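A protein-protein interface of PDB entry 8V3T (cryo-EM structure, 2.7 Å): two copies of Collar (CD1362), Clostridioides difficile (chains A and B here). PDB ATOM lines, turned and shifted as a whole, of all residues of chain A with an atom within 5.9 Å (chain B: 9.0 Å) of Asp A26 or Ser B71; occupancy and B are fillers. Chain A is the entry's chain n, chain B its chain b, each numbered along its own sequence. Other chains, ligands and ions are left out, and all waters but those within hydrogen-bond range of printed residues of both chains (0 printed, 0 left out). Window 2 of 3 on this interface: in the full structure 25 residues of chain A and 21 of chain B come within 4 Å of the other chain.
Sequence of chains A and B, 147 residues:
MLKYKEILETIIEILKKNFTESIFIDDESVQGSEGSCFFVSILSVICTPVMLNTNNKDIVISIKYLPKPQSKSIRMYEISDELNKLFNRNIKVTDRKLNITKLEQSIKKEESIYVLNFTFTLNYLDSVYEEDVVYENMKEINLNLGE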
ATOM      1  N   PHE A  24      -9.990 -18.145 -23.412  1.00  0.00           N
ATOM      2  CA  PHE A  24     -11.320 -17.887 -22.886  1.00  0.00           C
ATOM      3  C   PHE A  24     -11.975 -19.191 -22.451  1.00  0.00           C
ATOM      4  O   PHE A  24     -11.560 -20.283 -22.846  1.00  0.00           O
ATOM      5  CB  PHE A  24     -12.195 -17.175 -23.923  1.00  0.00           C
ATOM      6  CG  PHE A  24     -11.733 -15.786 -24.252  1.00  0.00           C
ATOM      7  CD1 PHE A  24     -11.363 -14.909 -23.247  1.00  0.00           C
ATOM      8  CD2 PHE A  24     -11.664 -15.357 -25.566  1.00  0.00           C
ATOM      9  CE1 PHE A  24     -10.936 -13.632 -23.547  1.00  0.00           C
ATOM     10  CE2 PHE A  24     -11.237 -14.080 -25.870  1.00  0.00           C
ATOM     11  CZ  PHE A  24     -10.873 -13.217 -24.859  1.00  0.00           C
ATOM     12  N   ILE A  25     -13.011 -19.061 -21.622  1.00  0.00           N
ATOM     13  CA  ILE A  25     -13.676 -20.212 -21.021  1.00  0.00           C
ATOM     14  C   ILE A  25     -15.151 -20.230 -21.411  1.00  0.00           C
ATOM     15  O   ILE A  25     -15.770 -21.297 -21.495  1.00  0.00           O
ATOM     16  CB  ILE A  25     -13.492 -20.202 -19.492  1.00  0.00           C
ATOM     17  CG1 ILE A  25     -12.035 -20.495 -19.145  1.00  0.00           C
ATOM     18  CG2 ILE A  25     -14.388 -21.218 -18.811  1.00  0.00           C
ATOM     19  CD1 ILE A  25     -11.661 -21.943 -19.344  1.00  0.00           C
ATOM     20  N   ASP A  26     -15.717 -19.059 -21.681  1.00  0.00           N
ATOM     21  CA  ASP A  26     -17.116 -18.942 -22.057  1.00  0.00           C
ATOM     22  C   ASP A  26     -17.247 -18.593 -23.534  1.00  0.00           C
ATOM     23  O   ASP A  26     -16.346 -18.008 -24.142  1.00  0.00           O
ATOM     24  CB  ASP A  26     -17.827 -17.884 -21.208  1.00  0.00           C
ATOM     25  CG  ASP A  26     -17.031 -16.603 -21.092  1.00  0.00           C
ATOM     26  OD1 ASP A  26     -15.792 -16.660 -21.228  1.00  0.00           O
ATOM     27  OD2 ASP A  26     -17.645 -15.540 -20.866  1.00  0.00           O
ATOM     28  N   ASP A  27     -18.390 -18.970 -24.108  1.00  0.00           N
ATOM     29  CA  ASP A  27     -18.657 -18.669 -25.511  1.00  0.00           C
ATOM     30  C   ASP A  27     -18.873 -17.180 -25.737  1.00  0.00           C
ATOM     31  O   ASP A  27     -18.607 -16.676 -26.834  1.00  0.00           O
ATOM     32  CB  ASP A  27     -19.873 -19.458 -25.993  1.00  0.00           C
ATOM     33  CG  ASP A  27     -19.995 -19.480 -27.504  1.00  0.00           C
ATOM     34  OD1 ASP A  27     -18.987 -19.212 -28.189  1.00  0.00           O
ATOM     35  OD2 ASP A  27     -21.101 -19.765 -28.007  1.00  0.00           O
ATOM     36  N   GLU A  28     -19.363 -16.465 -24.723  1.00  0.00           N
ATOM     37  CA  GLU A  28     -19.631 -15.038 -24.879  1.00  0.00           C
ATOM     38  C   GLU A  28     -18.350 -14.258 -25.137  1.00  0.00           C
ATOM     39  O   GLU A  28     -18.337 -13.321 -25.944  1.00  0.00           O
ATOM     40  CB  GLU A  28     -20.342 -14.504 -23.635  1.00  0.00           C
ATOM     41  CG  GLU A  28     -20.991 -13.144 -23.823  1.00  0.00           C
ATOM     42  CD  GLU A  28     -22.186 -13.188 -24.756  1.00  0.00           C
ATOM     43  OE1 GLU A  28     -22.717 -14.292 -24.999  1.00  0.00           O
ATOM     44  OE2 GLU A  28     -22.595 -12.116 -25.248  1.00  0.00           O
ATOM     45  N   SER A  29     -17.263 -14.625 -24.456  1.00  0.00           N
ATOM     46  CA  SER A  29     -16.020 -13.873 -24.582  1.00  0.00           C
ATOM     47  C   SER A  29     -15.380 -14.046 -25.954  1.00  0.00           C
ATOM     48  O   SER A  29     -14.755 -13.109 -26.462  1.00  0.00           O
ATOM     49  CB  SER A  29     -15.043 -14.295 -23.485  1.00  0.00           C
ATOM     50  OG  SER A  29     -14.128 -13.256 -23.191  1.00  0.00           O
ATOM     51  N   VAL A  30     -15.513 -15.226 -26.566  1.00  0.00           N
ATOM     52  CA  VAL A  30     -14.838 -15.466 -27.838  1.00  0.00           C
ATOM     53  C   VAL A  30     -15.491 -14.676 -28.967  1.00  0.00           C
ATOM     54  O   VAL A  30     -14.816 -14.291 -29.931  1.00  0.00           O
ATOM     55  CB  VAL A  30     -14.784 -16.976 -28.150  1.00  0.00           C
ATOM     56  CG1 VAL A  30     -14.401 -17.761 -26.906  1.00  0.00           C
ATOM     57  CG2 VAL A  30     -16.105 -17.474 -28.715  1.00  0.00           C
ATOM     58  N   PHE A  39     -10.245 -21.319 -26.904  1.00  0.00           N
ATOM     59  CA  PHE A  39     -11.375 -21.781 -26.107  1.00  0.00           C
ATOM     60  C   PHE A  39     -11.039 -23.133 -25.498  1.00  0.00           C
ATOM     61  O   PHE A  39     -10.648 -24.059 -26.214  1.00  0.00           O
ATOM     62  CB  PHE A  39     -12.651 -21.880 -26.946  1.00  0.00           C
ATOM     63  CG  PHE A  39     -13.867 -22.253 -26.150  1.00  0.00           C
ATOM     64  CD1 PHE A  39     -14.501 -21.315 -25.354  1.00  0.00           C
ATOM     65  CD2 PHE A  39     -14.370 -23.540 -26.188  1.00  0.00           C
ATOM     66  CE1 PHE A  39     -15.616 -21.655 -24.616  1.00  0.00           C
ATOM     67  CE2 PHE A  39     -15.487 -23.883 -25.451  1.00  0.00           C
ATOM     68  CZ  PHE A  39     -16.110 -22.939 -24.664  1.00  0.00           C
ATOM     69  N   VAL A  40     -11.204 -23.246 -24.182  1.00  0.00           N
ATOM     70  CA  VAL A  40     -10.841 -24.442 -23.432  1.00  0.00           C
ATOM     71  C   VAL A  40     -12.048 -24.898 -22.626  1.00  0.00           C
ATOM     72  O   VAL A  40     -12.711 -24.080 -21.979  1.00  0.00           O
ATOM     73  CB  VAL A  40      -9.639 -24.191 -22.500  1.00  0.00           C
ATOM     74  CG1 VAL A  40      -9.212 -25.482 -21.824  1.00  0.00           C
ATOM     75  CG2 VAL A  40      -8.485 -23.583 -23.273  1.00  0.00           C
ATOM     76  N   SER B  36     -29.078 -18.696 -13.250  1.00  0.00           N
ATOM     77  CA  SER B  36     -28.400 -19.816 -12.593  1.00  0.00           C
ATOM     78  C   SER B  36     -29.391 -20.725 -11.859  1.00  0.00           C
ATOM     79  O   SER B  36     -29.397 -20.835 -10.633  1.00  0.00           O
ATOM     80  CB  SER B  36     -27.311 -19.301 -11.644  1.00  0.00           C
ATOM     81  OG  SER B  36     -26.109 -19.044 -12.347  1.00  0.00           O
ATOM     82  N   TYR B  65     -27.425 -27.707 -15.025  1.00  0.00           N
ATOM     83  CA  TYR B  65     -27.186 -26.375 -14.484  1.00  0.00           C
ATOM     84  C   TYR B  65     -27.032 -25.404 -15.644  1.00  0.00           C
ATOM     85  O   TYR B  65     -26.152 -25.581 -16.493  1.00  0.00           O
ATOM     86  CB  TYR B  65     -25.947 -26.354 -13.589  1.00  0.00           C
ATOM     87  CG  TYR B  65     -25.562 -24.970 -13.123  1.00  0.00           C
ATOM     88  CD1 TYR B  65     -26.294 -24.321 -12.139  1.00  0.00           C
ATOM     89  CD2 TYR B  65     -24.464 -24.315 -13.661  1.00  0.00           C
ATOM     90  CE1 TYR B  65     -25.949 -23.056 -11.712  1.00  0.00           C
ATOM     91  CE2 TYR B  65     -24.109 -23.052 -13.238  1.00  0.00           C
ATOM     92  CZ  TYR B  65     -24.854 -22.428 -12.262  1.00  0.00           C
ATOM     93  OH  TYR B  65     -24.506 -21.168 -11.835  1.00  0.00           O
ATOM     94  N   PRO B  67     -26.334 -21.532 -16.604  1.00  0.00           N
ATOM     95  CA  PRO B  67     -25.943 -20.183 -16.173  1.00  0.00           C
ATOM     96  C   PRO B  67     -26.518 -19.119 -17.096  1.00  0.00           C
ATOM     97  O   PRO B  67     -26.115 -18.995 -18.256  1.00  0.00           O
ATOM     98  CB  PRO B  67     -24.410 -20.234 -16.238  1.00  0.00           C
ATOM     99  CG  PRO B  67     -24.090 -21.309 -17.235  1.00  0.00           C
ATOM    100  CD  PRO B  67     -25.308 -22.170 -17.444  1.00  0.00           C
ATOM    101  N   LYS B  68     -27.475 -18.345 -16.576  1.00  0.00           N
ATOM    102  CA  LYS B  68     -28.040 -17.254 -17.370  1.00  0.00           C
ATOM    103  C   LYS B  68     -27.125 -16.037 -17.422  1.00  0.00           C
ATOM    104  O   LYS B  68     -26.875 -15.530 -18.529  1.00  0.00           O
ATOM    105  CB  LYS B  68     -29.433 -16.890 -16.846  1.00  0.00           C
ATOM    106  CG  LYS B  68     -30.112 -15.776 -17.623  1.00  0.00           C
ATOM    107  CD  LYS B  68     -31.598 -16.034 -17.782  1.00  0.00           C
ATOM    108  CE  LYS B  68     -31.860 -17.310 -18.555  1.00  0.00           C
ATOM    109  NZ  LYS B  68     -33.262 -17.365 -19.054  1.00  0.00           N
ATOM    110  N   PRO B  69     -26.612 -15.506 -16.308  1.00  0.00           N
ATOM    111  CA  PRO B  69     -25.741 -14.331 -16.406  1.00  0.00           C
ATOM    112  C   PRO B  69     -24.429 -14.662 -17.097  1.00  0.00           C
ATOM    113  O   PRO B  69     -23.951 -15.798 -17.070  1.00  0.00           O
ATOM    114  CB  PRO B  69     -25.512 -13.925 -14.945  1.00  0.00           C
ATOM    115  CG  PRO B  69     -25.820 -15.138 -14.155  1.00  0.00           C
ATOM    116  CD  PRO B  69     -26.886 -15.857 -14.902  1.00  0.00           C
ATOM    117  N   GLN B  70     -23.856 -13.647 -17.732  1.00  0.00           N
ATOM    118  CA  GLN B  70     -22.607 -13.819 -18.458  1.00  0.00           C
ATOM    119  C   GLN B  70     -21.448 -14.076 -17.498  1.00  0.00           C
ATOM    120  O   GLN B  70     -21.443 -13.609 -16.356  1.00  0.00           O
ATOM    121  CB  GLN B  70     -22.324 -12.583 -19.312  1.00  0.00           C
ATOM    122  CG  GLN B  70     -22.242 -11.286 -18.518  1.00  0.00           C
ATOM    123  CD  GLN B  70     -22.242 -10.055 -19.405  1.00  0.00           C
ATOM    124  OE1 GLN B  70     -22.312 -10.159 -20.629  1.00  0.00           O
ATOM    125  NE2 GLN B  70     -22.162  -8.881 -18.789  1.00  0.00           N
ATOM    126  N   SER B  71     -20.466 -14.845 -17.979  1.00  0.00           N
ATOM    127  CA  SER B  71     -19.225 -15.122 -17.249  1.00  0.00           C
ATOM    128  C   SER B  71     -19.484 -15.909 -15.963  1.00  0.00           C
ATOM    129  O   SER B  71     -19.092 -15.502 -14.869  1.00  0.00           O
ATOM    130  CB  SER B  71     -18.459 -13.828 -16.956  1.00  0.00           C
ATOM    131  OG  SER B  71     -19.036 -13.126 -15.868  1.00  0.00           O
ATOM    132  N   LYS B  72     -20.152 -17.056 -16.105  1.00  0.00           N
ATOM    133  CA  LYS B  72     -20.459 -17.932 -14.977  1.00  0.00           C
ATOM    134  C   LYS B  72     -19.992 -19.369 -15.200  1.00  0.00           C
ATOM    135  O   LYS B  72     -20.545 -20.292 -14.594  1.00  0.00           O
ATOM    136  CB  LYS B  72     -21.960 -17.913 -14.682  1.00  0.00           C
ATOM    137  CG  LYS B  72     -22.520 -16.558 -14.277  1.00  0.00           C
ATOM    138  CD  LYS B  72     -21.712 -15.923 -13.162  1.00  0.00           C
ATOM    139  CE  LYS B  72     -22.137 -14.483 -12.926  1.00  0.00           C
ATOM    140  NZ  LYS B  72     -21.983 -13.643 -14.144  1.00  0.00           N
ATOM    141  N   SER B  73     -18.994 -19.585 -16.059  1.00  0.00           N
ATOM    142  CA  SER B  73     -18.556 -20.945 -16.361  1.00  0.00           C
ATOM    143  C   SER B  73     -17.680 -21.540 -15.262  1.00  0.00           C
ATOM    144  O   SER B  73     -17.706 -22.759 -15.039  1.00  0.00           O
ATOM    145  CB  SER B  73     -17.812 -20.969 -17.696  1.00  0.00           C
ATOM    146  OG  SER B  73     -18.721 -21.012 -18.780  1.00  0.00           O
ATOM    147  N   ILE B  74     -16.894 -20.715 -14.572  1.00  0.00           N
ATOM    148  CA  ILE B  74     -16.075 -21.245 -13.489  1.00  0.00           C
ATOM    149  C   ILE B  74     -16.972 -21.779 -12.377  1.00  0.00           C
ATOM    150  O   ILE B  74     -16.641 -22.763 -11.698  1.00  0.00           O
ATOM    151  CB  ILE B  74     -15.092 -20.169 -12.992  1.00  0.00           C
ATOM    152  CG1 ILE B  74     -14.101 -20.778 -12.003  1.00  0.00           C
ATOM    153  CG2 ILE B  74     -15.830 -18.989 -12.381  1.00  0.00           C
ATOM    154  CD1 ILE B  74     -13.402 -21.995 -12.563  1.00  0.00           C
ATOM    155  N   ARG B  75     -18.136 -21.153 -12.189  1.00  0.00           N
ATOM    156  CA  ARG B  75     -19.153 -21.727 -11.321  1.00  0.00           C
ATOM    157  C   ARG B  75     -19.623 -23.076 -11.845  1.00  0.00           C
ATOM    158  O   ARG B  75     -19.895 -23.990 -11.055  1.00  0.00           O
ATOM    159  CB  ARG B  75     -20.332 -20.764 -11.192  1.00  0.00           C
ATOM    160  CG  ARG B  75     -21.300 -21.128 -10.091  1.00  0.00           C
ATOM    161  CD  ARG B  75     -20.721 -20.786  -8.734  1.00  0.00           C
ATOM    162  NE  ARG B  75     -21.655 -21.077  -7.653  1.00  0.00           N
ATOM    163  CZ  ARG B  75     -21.653 -22.199  -6.947  1.00  0.00           C
ATOM    164  NH1 ARG B  75     -20.768 -23.155  -7.172  1.00  0.00           N
ATOM    165  NH2 ARG B  75     -22.559 -22.363  -5.989  1.00  0.00           N
ATOM    166  N   MET B  76     -19.724 -23.220 -13.170  1.00  0.00           N
ATOM    167  CA  MET B  76     -20.075 -24.510 -13.752  1.00  0.00           C
ATOM    168  C   MET B  76     -19.038 -25.568 -13.412  1.00  0.00           C
ATOM    169  O   MET B  76     -19.378 -26.748 -13.269  1.00  0.00           O
ATOM    170  CB  MET B  76     -20.218 -24.386 -15.269  1.00  0.00           C
ATOM    171  CG  MET B  76     -21.212 -25.338 -15.895  1.00  0.00           C
ATOM    172  SD  MET B  76     -21.501 -25.013 -17.645  1.00  0.00           S
ATOM    173  CE  MET B  76     -19.890 -24.422 -18.158  1.00  0.00           C
ATOM    174  N   TYR B  77     -17.775 -25.169 -13.271  1.00  0.00           N
ATOM    175  CA  TYR B  77     -16.729 -26.126 -12.927  1.00  0.00           C
ATOM    176  C   TYR B  77     -16.625 -26.405 -11.431  1.00  0.00           C
ATOM    177  O   TYR B  77     -16.116 -27.465 -11.052  1.00  0.00           O
ATOM    178  CB  TYR B  77     -15.377 -25.645 -13.463  1.00  0.00           C
ATOM    179  CG  TYR B  77     -15.252 -25.806 -14.961  1.00  0.00           C
ATOM    180  CD1 TYR B  77     -15.007 -27.050 -15.523  1.00  0.00           C
ATOM    181  CD2 TYR B  77     -15.407 -24.723 -15.813  1.00  0.00           C
ATOM    182  CE1 TYR B  77     -14.904 -27.208 -16.890  1.00  0.00           C
ATOM    183  CE2 TYR B  77     -15.306 -24.872 -17.180  1.00  0.00           C
ATOM    184  CZ  TYR B  77     -15.054 -26.116 -17.712  1.00  0.00           C
ATOM    185  OH  TYR B  77     -14.952 -26.270 -19.074  1.00  0.00           O
ATOM    186  N   LYS B 109     -23.052 -27.103 -25.766  1.00  0.00           N
ATOM    187  CA  LYS B 109     -23.846 -25.900 -25.957  1.00  0.00           C
ATOM    188  C   LYS B 109     -25.220 -26.281 -26.487  1.00  0.00           C
ATOM    189  O   LYS B 109     -25.337 -27.043 -27.455  1.00  0.00           O
ATOM    190  CB  LYS B 109     -23.129 -24.904 -26.880  1.00  0.00           C
ATOM    191  CG  LYS B 109     -23.327 -25.086 -28.375  1.00  0.00           C
ATOM    192  CD  LYS B 109     -22.542 -24.049 -29.162  1.00  0.00           C
ATOM    193  CE  LYS B 109     -22.847 -22.642 -28.684  1.00  0.00           C
ATOM    194  NZ  LYS B 109     -22.045 -21.624 -29.416  1.00  0.00           N
ATOM    195  N   SER B 112     -27.557 -21.208 -28.060  1.00  0.00           N
ATOM    196  CA  SER B 112     -26.396 -20.329 -28.056  1.00  0.00           C
ATOM    197  C   SER B 112     -25.543 -20.418 -26.793  1.00  0.00           C
ATOM    198  O   SER B 112     -24.492 -19.772 -26.739  1.00  0.00           O
ATOM    199  CB  SER B 112     -26.841 -18.875 -28.248  1.00  0.00           C
ATOM    200  OG  SER B 112     -27.841 -18.524 -27.308  1.00  0.00           O
ATOM    201  N   ILE B 113     -25.948 -21.188 -25.784  1.00  0.00           N
ATOM    202  CA  ILE B 113     -25.285 -21.171 -24.484  1.00  0.00           C
ATOM    203  C   ILE B 113     -24.806 -22.572 -24.122  1.00  0.00           C
ATOM    204  O   ILE B 113     -25.474 -23.569 -24.416  1.00  0.00           O
ATOM    205  CB  ILE B 113     -26.204 -20.594 -23.382  1.00  0.00           C
ATOM    206  CG1 ILE B 113     -27.211 -21.633 -22.885  1.00  0.00           C
ATOM    207  CG2 ILE B 113     -26.918 -19.345 -23.877  1.00  0.00           C
ATOM    208  CD1 ILE B 113     -27.638 -21.431 -21.449  1.00  0.00           C
ATOM    209  N   TYR B 114     -23.617 -22.640 -23.526  1.00  0.00           N
ATOM    210  CA  TYR B 114     -23.099 -23.889 -22.982  1.00  0.00           C
ATOM    211  C   TYR B 114     -23.773 -24.218 -21.655  1.00  0.00           C
ATOM    212  O   TYR B 114     -24.072 -23.328 -20.855  1.00  0.00           O
ATOM    213  CB  TYR B 114     -21.587 -23.794 -22.787  1.00  0.00           C
ATOM    214  CG  TYR B 114     -20.782 -23.980 -24.051  1.00  0.00           C
ATOM    215  CD1 TYR B 114     -20.427 -25.248 -24.492  1.00  0.00           C
ATOM    216  CD2 TYR B 114     -20.376 -22.889 -24.806  1.00  0.00           C
ATOM    217  CE1 TYR B 114     -19.692 -25.422 -25.645  1.00  0.00           C
ATOM    218  CE2 TYR B 114     -19.639 -23.055 -25.961  1.00  0.00           C
ATOM    219  CZ  TYR B 114     -19.299 -24.323 -26.376  1.00  0.00           C
ATOM    220  OH  TYR B 114     -18.566 -24.493 -27.527  1.00  0.00           O
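OD2 of Asp A27 lies within salt-bridge range of NZ of Lys B109 (2.5 Å).
No position is printed for both chains.
Among the printed residues, merely in contact across the chains: Asp A27 with Tyr B114 (3.6 Å), Ile A25 with Ser B73 (3.6 Å), Asp A27 with Ser B112 (3.6 Å), Phe A39 with Tyr B114 (3.8 Å) and Asp A26 with Ser B71 (3.97 Å).
Of the printed residues of chain B, Ile A25 touches Ser B73. Printed residues of chain B within 4 Å of Asp A27: Lys B109 (2.5 Å), Ser B112 (3.6 Å) and Tyr B114 (3.6 Å). Of the printed residues of chain B, Phe A39 touches Tyr B114. Printed residues of chain A within 4 Å of Tyr B114: Asp A27 (3.6 Å) and Phe A39 (3.8 Å).
Of the 9 printed residues of chain A, 4 touch a printed residue of chain B. Hydrophobic or aromatic side chains of chain A that line the printed part of chain B: Ile A25 and Phe A39. Printed residues of chain B that touch a printed residue of chain A: Ser B71, Ser B73, Lys B109, Ser B112 and Tyr B114. Hydrophobic or aromatic side chains of chain B within 4 Å of the printed part of chain A: Tyr B114.
NZ of Lys B72 lies within hydrogen-bond range of OG of Ser B71 (3.5 Å).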
